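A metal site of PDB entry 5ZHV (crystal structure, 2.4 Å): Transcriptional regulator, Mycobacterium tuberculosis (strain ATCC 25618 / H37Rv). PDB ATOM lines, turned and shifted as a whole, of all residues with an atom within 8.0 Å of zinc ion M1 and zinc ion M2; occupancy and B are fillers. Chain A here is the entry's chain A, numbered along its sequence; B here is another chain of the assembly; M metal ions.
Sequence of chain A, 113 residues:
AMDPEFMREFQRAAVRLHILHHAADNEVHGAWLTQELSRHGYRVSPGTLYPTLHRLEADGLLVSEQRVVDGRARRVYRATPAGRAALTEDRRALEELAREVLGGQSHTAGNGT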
ATOM      1  N   ALA A  14      20.714  -9.792  14.038  1.00  0.00           N
ATOM      2  CA  ALA A  14      21.225 -11.057  14.567  1.00  0.00           C
ATOM      3  C   ALA A  14      20.285 -11.657  15.624  1.00  0.00           C
ATOM      4  O   ALA A  14      20.016 -12.863  15.643  1.00  0.00           O
ATOM      5  CB  ALA A  14      22.610 -10.832  15.138  1.00  0.00           C
ATOM      6  N   HIS A  18      18.081 -15.047  15.575  1.00  0.00           N
ATOM      7  CA  HIS A  18      18.221 -16.061  16.639  1.00  0.00           C
ATOM      8  C   HIS A  18      16.905 -16.397  17.294  1.00  0.00           C
ATOM      9  O   HIS A  18      16.668 -17.546  17.603  1.00  0.00           O
ATOM     10  CB  HIS A  18      19.235 -15.647  17.714  1.00  0.00           C
ATOM     11  CG  HIS A  18      20.632 -16.080  17.415  1.00  0.00           C
ATOM     12  ND1 HIS A  18      21.486 -15.327  16.631  1.00  0.00           N
ATOM     13  CD2 HIS A  18      21.326 -17.193  17.773  1.00  0.00           C
ATOM     14  CE1 HIS A  18      22.636 -15.948  16.514  1.00  0.00           C
ATOM     15  NE2 HIS A  18      22.576 -17.072  17.205  1.00  0.00           N
ATOM     16  N   HIS A  21      15.056 -18.597  14.954  1.00  0.00           N
ATOM     17  CA  HIS A  21      15.628 -19.897  14.771  1.00  0.00           C
ATOM     18  C   HIS A  21      15.311 -20.763  15.985  1.00  0.00           C
ATOM     19  O   HIS A  21      14.903 -21.902  15.818  1.00  0.00           O
ATOM     20  CB  HIS A  21      17.100 -19.883  14.402  1.00  0.00           C
ATOM     21  CG  HIS A  21      17.687 -21.269  14.344  1.00  0.00           C
ATOM     22  ND1 HIS A  21      18.899 -21.605  14.918  1.00  0.00           N
ATOM     23  CD2 HIS A  21      17.200 -22.417  13.796  1.00  0.00           C
ATOM     24  CE1 HIS A  21      19.127 -22.896  14.736  1.00  0.00           C
ATOM     25  NE2 HIS A  21      18.117 -23.413  14.063  1.00  0.00           N
ATOM     26  N   HIS A  22      15.458 -20.211  17.182  1.00  0.00           N
ATOM     27  CA  HIS A  22      15.101 -20.934  18.394  1.00  0.00           C
ATOM     28  C   HIS A  22      13.621 -21.290  18.447  1.00  0.00           C
ATOM     29  O   HIS A  22      13.295 -22.412  18.792  1.00  0.00           O
ATOM     30  CB  HIS A  22      15.544 -20.186  19.664  1.00  0.00           C
ATOM     31  CG  HIS A  22      17.026 -20.194  19.870  1.00  0.00           C
ATOM     32  ND1 HIS A  22      17.850 -19.227  19.337  1.00  0.00           N
ATOM     33  CD2 HIS A  22      17.829 -21.077  20.512  1.00  0.00           C
ATOM     34  CE1 HIS A  22      19.106 -19.497  19.663  1.00  0.00           C
ATOM     35  NE2 HIS A  22      19.119 -20.608  20.381  1.00  0.00           N
ATOM     36  N   ASP A  25      12.759 -24.303  16.136  1.00  0.00           N
ATOM     37  CA  ASP A  25      13.263 -25.578  16.647  1.00  0.00           C
ATOM     38  C   ASP A  25      12.379 -26.193  17.737  1.00  0.00           C
ATOM     39  O   ASP A  25      12.195 -27.407  17.788  1.00  0.00           O
ATOM     40  CB  ASP A  25      14.710 -25.455  17.165  1.00  0.00           C
ATOM     41  CG  ASP A  25      15.753 -25.695  16.056  1.00  0.00           C
ATOM     42  OD1 ASP A  25      15.404 -26.211  14.958  1.00  0.00           O
ATOM     43  OD2 ASP A  25      16.947 -25.347  16.271  1.00  0.00           O
ATOM     44  N   ASN A  26      11.812 -25.319  18.574  1.00  0.00           N
ATOM     45  CA  ASN A  26      11.078 -25.698  19.771  1.00  0.00           C
ATOM     46  C   ASN A  26      10.334 -24.484  20.338  1.00  0.00           C
ATOM     47  O   ASN A  26      10.591 -23.355  19.958  1.00  0.00           O
ATOM     48  CB  ASN A  26      12.056 -26.317  20.808  1.00  0.00           C
ATOM     49  CG  ASN A  26      13.112 -25.333  21.353  1.00  0.00           C
ATOM     50  OD1 ASN A  26      14.036 -24.913  20.633  1.00  0.00           O
ATOM     51  ND2 ASN A  26      12.980 -24.976  22.611  1.00  0.00           N
ATOM     52  N   TRP A  32      13.824 -17.836  29.200  1.00  0.00           N
ATOM     53  CA  TRP A  32      14.837 -18.703  28.622  1.00  0.00           C
ATOM     54  C   TRP A  32      15.535 -18.091  27.402  1.00  0.00           C
ATOM     55  O   TRP A  32      16.755 -18.221  27.254  1.00  0.00           O
ATOM     56  CB  TRP A  32      14.257 -20.042  28.265  1.00  0.00           C
ATOM     57  CG  TRP A  32      15.286 -21.016  27.774  1.00  0.00           C
ATOM     58  CD1 TRP A  32      16.164 -21.734  28.536  1.00  0.00           C
ATOM     59  CD2 TRP A  32      15.552 -21.366  26.418  1.00  0.00           C
ATOM     60  NE1 TRP A  32      16.947 -22.519  27.744  1.00  0.00           N
ATOM     61  CE2 TRP A  32      16.600 -22.325  26.431  1.00  0.00           C
ATOM     62  CE3 TRP A  32      15.001 -20.975  25.189  1.00  0.00           C
ATOM     63  CZ2 TRP A  32      17.114 -22.928  25.262  1.00  0.00           C
ATOM     64  CZ3 TRP A  32      15.504 -21.571  24.016  1.00  0.00           C
ATOM     65  CH2 TRP A  32      16.562 -22.538  24.063  1.00  0.00           C
ATOM     66  N   LEU A  33      14.777 -17.411  26.534  1.00  0.00           N
ATOM     67  CA  LEU A  33      15.368 -16.690  25.422  1.00  0.00           C
ATOM     68  C   LEU A  33      16.440 -15.715  25.870  1.00  0.00           C
ATOM     69  O   LEU A  33      17.491 -15.656  25.251  1.00  0.00           O
ATOM     70  CB  LEU A  33      14.303 -15.947  24.609  1.00  0.00           C
ATOM     71  CG  LEU A  33      13.662 -16.697  23.469  1.00  0.00           C
ATOM     72  CD1 LEU A  33      12.725 -15.760  22.734  1.00  0.00           C
ATOM     73  CD2 LEU A  33      14.667 -17.351  22.499  1.00  0.00           C
ATOM     74  N   GLN A  35      18.373 -15.873  28.554  1.00  0.00           N
ATOM     75  CA  GLN A  35      19.554 -16.699  28.874  1.00  0.00           C
ATOM     76  C   GLN A  35      20.233 -17.241  27.622  1.00  0.00           C
ATOM     77  O   GLN A  35      21.446 -17.194  27.503  1.00  0.00           O
ATOM     78  CB  GLN A  35      19.204 -17.872  29.803  1.00  0.00           C
ATOM     79  CG  GLN A  35      18.347 -17.522  31.036  1.00  0.00           C
ATOM     80  CD  GLN A  35      19.172 -16.900  32.166  1.00  0.00           C
ATOM     81  OE1 GLN A  35      19.771 -15.829  32.003  1.00  0.00           O
ATOM     82  NE2 GLN A  35      19.234 -17.597  33.327  1.00  0.00           N
ATOM     83  N   GLU A  36      19.445 -17.743  26.684  1.00  0.00           N
ATOM     84  CA  GLU A  36      19.982 -18.318  25.461  1.00  0.00           C
ATOM     85  C   GLU A  36      20.698 -17.332  24.583  1.00  0.00           C
ATOM     86  O   GLU A  36      21.753 -17.635  24.026  1.00  0.00           O
ATOM     87  CB  GLU A  36      18.863 -19.014  24.674  1.00  0.00           C
ATOM     88  CG  GLU A  36      18.953 -20.515  24.743  1.00  0.00           C
ATOM     89  CD  GLU A  36      20.319 -21.093  24.402  1.00  0.00           C
ATOM     90  OE1 GLU A  36      20.903 -20.655  23.390  1.00  0.00           O
ATOM     91  OE2 GLU A  36      20.778 -21.994  25.134  1.00  0.00           O
ATOM     92  N   LEU A  37      20.109 -16.136  24.456  1.00  0.00           N
ATOM     93  CA  LEU A  37      20.700 -15.053  23.690  1.00  0.00           C
ATOM     94  C   LEU A  37      22.014 -14.623  24.331  1.00  0.00           C
ATOM     95  O   LEU A  37      23.014 -14.443  23.627  1.00  0.00           O
ATOM     96  CB  LEU A  37      19.735 -13.895  23.536  1.00  0.00           C
ATOM     97  CG  LEU A  37      18.572 -14.186  22.563  1.00  0.00           C
ATOM     98  CD1 LEU A  37      17.420 -13.203  22.739  1.00  0.00           C
ATOM     99  CD2 LEU A  37      18.992 -14.283  21.084  1.00  0.00           C
ATOM    100  N   ARG A  39      24.005 -16.575  26.174  1.00  0.00           N
ATOM    101  CA  ARG A  39      24.961 -17.625  25.793  1.00  0.00           C
ATOM    102  C   ARG A  39      25.552 -17.396  24.398  1.00  0.00           C
ATOM    103  O   ARG A  39      26.747 -17.599  24.203  1.00  0.00           O
ATOM    104  CB  ARG A  39      24.337 -19.026  25.874  1.00  0.00           C
ATOM    105  CG  ARG A  39      24.367 -19.681  27.237  1.00  0.00           C
ATOM    106  CD  ARG A  39      23.826 -21.124  27.194  1.00  0.00           C
ATOM    107  NE  ARG A  39      22.365 -21.167  27.103  1.00  0.00           N
ATOM    108  CZ  ARG A  39      21.514 -21.203  28.139  1.00  0.00           C
ATOM    109  NH1 ARG A  39      21.977 -21.211  29.391  1.00  0.00           N
ATOM    110  NH2 ARG A  39      20.194 -21.236  27.927  1.00  0.00           N
ATOM    111  N   HIS A  40      24.730 -16.946  23.454  1.00  0.00           N
ATOM    112  CA  HIS A  40      25.203 -16.698  22.096  1.00  0.00           C
ATOM    113  C   HIS A  40      25.964 -15.370  21.955  1.00  0.00           C
ATOM    114  O   HIS A  40      26.403 -15.034  20.863  1.00  0.00           O
ATOM    115  CB  HIS A  40      24.040 -16.762  21.110  1.00  0.00           C
ATOM    116  CG  HIS A  40      23.570 -18.149  20.797  1.00  0.00           C
ATOM    117  ND1 HIS A  40      24.260 -19.007  19.966  1.00  0.00           N
ATOM    118  CD2 HIS A  40      22.441 -18.807  21.158  1.00  0.00           C
ATOM    119  CE1 HIS A  40      23.589 -20.141  19.849  1.00  0.00           C
ATOM    120  NE2 HIS A  40      22.476 -20.050  20.554  1.00  0.00           N
ATOM    121  N   GLY A  41      26.093 -14.628  23.050  1.00  0.00           N
ATOM    122  CA  GLY A  41      26.869 -13.392  23.078  1.00  0.00           C
ATOM    123  C   GLY A  41      26.119 -12.098  22.780  1.00  0.00           C
ATOM    124  O   GLY A  41      26.717 -11.140  22.294  1.00  0.00           O
ATOM    125  N   TYR A  42      24.824 -12.045  23.068  1.00  0.00           N
ATOM    126  CA  TYR A  42      24.047 -10.826  22.837  1.00  0.00           C
ATOM    127  C   TYR A  42      23.498 -10.286  24.147  1.00  0.00           C
ATOM    128  O   TYR A  42      22.834 -11.003  24.913  1.00  0.00           O
ATOM    129  CB  TYR A  42      22.955 -11.043  21.784  1.00  0.00           C
ATOM    130  CG  TYR A  42      23.479 -11.580  20.455  1.00  0.00           C
ATOM    131  CD1 TYR A  42      24.047 -10.727  19.478  1.00  0.00           C
ATOM    132  CD2 TYR A  42      23.445 -12.946  20.187  1.00  0.00           C
ATOM    133  CE1 TYR A  42      24.539 -11.245  18.259  1.00  0.00           C
ATOM    134  CE2 TYR A  42      23.926 -13.463  18.978  1.00  0.00           C
ATOM    135  CZ  TYR A  42      24.482 -12.625  18.042  1.00  0.00           C
ATOM    136  OH  TYR A  42      24.958 -13.196  16.889  1.00  0.00           O
ATOM    137  N   GLU B  96      31.072 -14.773  11.419  1.00  0.00           N
ATOM    138  CA  GLU B  96      30.703 -15.561  12.585  1.00  0.00           C
ATOM    139  C   GLU B  96      29.262 -16.013  12.453  1.00  0.00           C
ATOM    140  O   GLU B  96      29.004 -17.219  12.516  1.00  0.00           O
ATOM    141  CB  GLU B  96      30.910 -14.791  13.878  1.00  0.00           C
ATOM    142  CG  GLU B  96      32.358 -14.795  14.363  1.00  0.00           C
ATOM    143  CD  GLU B  96      32.525 -14.194  15.766  1.00  0.00           C
ATOM    144  OE1 GLU B  96      31.865 -14.662  16.731  1.00  0.00           O
ATOM    145  OE2 GLU B  96      33.354 -13.260  15.910  1.00  0.00           O
ATOM    146  N   LEU B  97      28.359 -15.042  12.206  1.00  0.00           N
ATOM    147  CA  LEU B  97      26.936 -15.330  12.110  1.00  0.00           C
ATOM    148  C   LEU B  97      26.596 -16.213  10.921  1.00  0.00           C
ATOM    149  O   LEU B  97      25.741 -17.111  11.029  1.00  0.00           O
ATOM    150  CB  LEU B  97      26.116 -14.040  12.085  1.00  0.00           C
ATOM    151  CG  LEU B  97      24.610 -14.214  12.156  1.00  0.00           C
ATOM    152  CD1 LEU B  97      24.218 -14.909  13.451  1.00  0.00           C
ATOM    153  CD2 LEU B  97      23.909 -12.871  12.052  1.00  0.00           C
ATOM    154  N   GLU B 100      27.623 -19.801  11.798  1.00  0.00           N
ATOM    155  CA  GLU B 100      26.703 -20.368  12.788  1.00  0.00           C
ATOM    156  C   GLU B 100      25.389 -20.912  12.197  1.00  0.00           C
ATOM    157  O   GLU B 100      24.969 -22.009  12.571  1.00  0.00           O
ATOM    158  CB  GLU B 100      26.411 -19.316  13.847  1.00  0.00           C
ATOM    159  CG  GLU B 100      25.632 -19.786  15.061  1.00  0.00           C
ATOM    160  CD  GLU B 100      25.177 -18.617  15.933  1.00  0.00           C
ATOM    161  OE1 GLU B 100      24.503 -18.874  16.954  1.00  0.00           O
ATOM    162  OE2 GLU B 100      25.485 -17.437  15.634  1.00  0.00           O
ATOM    163  N   VAL B 101      24.766 -20.172  11.289  1.00  0.00           N
ATOM    164  CA  VAL B 101      23.426 -20.547  10.801  1.00  0.00           C
ATOM    165  C   VAL B 101      23.355 -21.214   9.430  1.00  0.00           C
ATOM    166  O   VAL B 101      22.307 -21.682   9.046  1.00  0.00           O
ATOM    167  CB  VAL B 101      22.387 -19.391  10.936  1.00  0.00           C
ATOM    168  CG1 VAL B 101      22.280 -18.935  12.387  1.00  0.00           C
ATOM    169  CG2 VAL B 101      22.720 -18.232  10.011  1.00  0.00           C
HETATM  170 ZN    ZN M   1      20.933 -21.733  21.201  1.00  0.00          ZN
HETATM  171 ZN    ZN M   2      24.908 -17.279  18.021  1.00  0.00          ZN
HETATM  172 ZN    ZN M   3      20.330 -20.197  14.730  1.00  0.00          ZN
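Zinc ion M1 is bound by a ring nitrogen (NE2) of His 22 (2.3 Å), a ring nitrogen (NE2) of His 40 (2.4 Å) and the side-chain carboxylate of Glu 36 (2.4 Å).
Three residues have an atom within 4 Å of zinc ion M1: His 22, Glu 36 and His 40.
A ring nitrogen (ND1) of His 18 is in hydrogen-bond range of the backbone carbonyl oxygen of Ala 14. ND1 of His 22 is in hydrogen-bond range of O of His 18 (2.7 Å). The side-chain carboxylate (OE2) of Glu 36 is in salt-bridge range of the guanidinium group (NE) of Arg 39. The backbone carbonyl oxygen (O) of His 22 lies close to the side-chain amide oxygen (OD1) of Asn 26 (3.2 Å).
OE1 of Glu 100 of chain B binds zinc ion M2 (2.0 Å). OE2 of Glu 100 of chain B binds zinc ion M2, at 2.5 Å. NE2 of His 18 binds zinc ion M2 (2.5 Å). ND1 of His 40 binds zinc ion M2, at 2.7 Å. Zinc ion M2 has four donor atoms within binding distance.
Within 4 Å of zinc ion M2: His 18, His 40 and Glu 100 of chain B. Along chain A the residues within 4 Å of zinc ion M2 span positions 18 to 40. The nearest printed residue that does not touch zinc ion M2 is Tyr 42 (4.1 Å).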
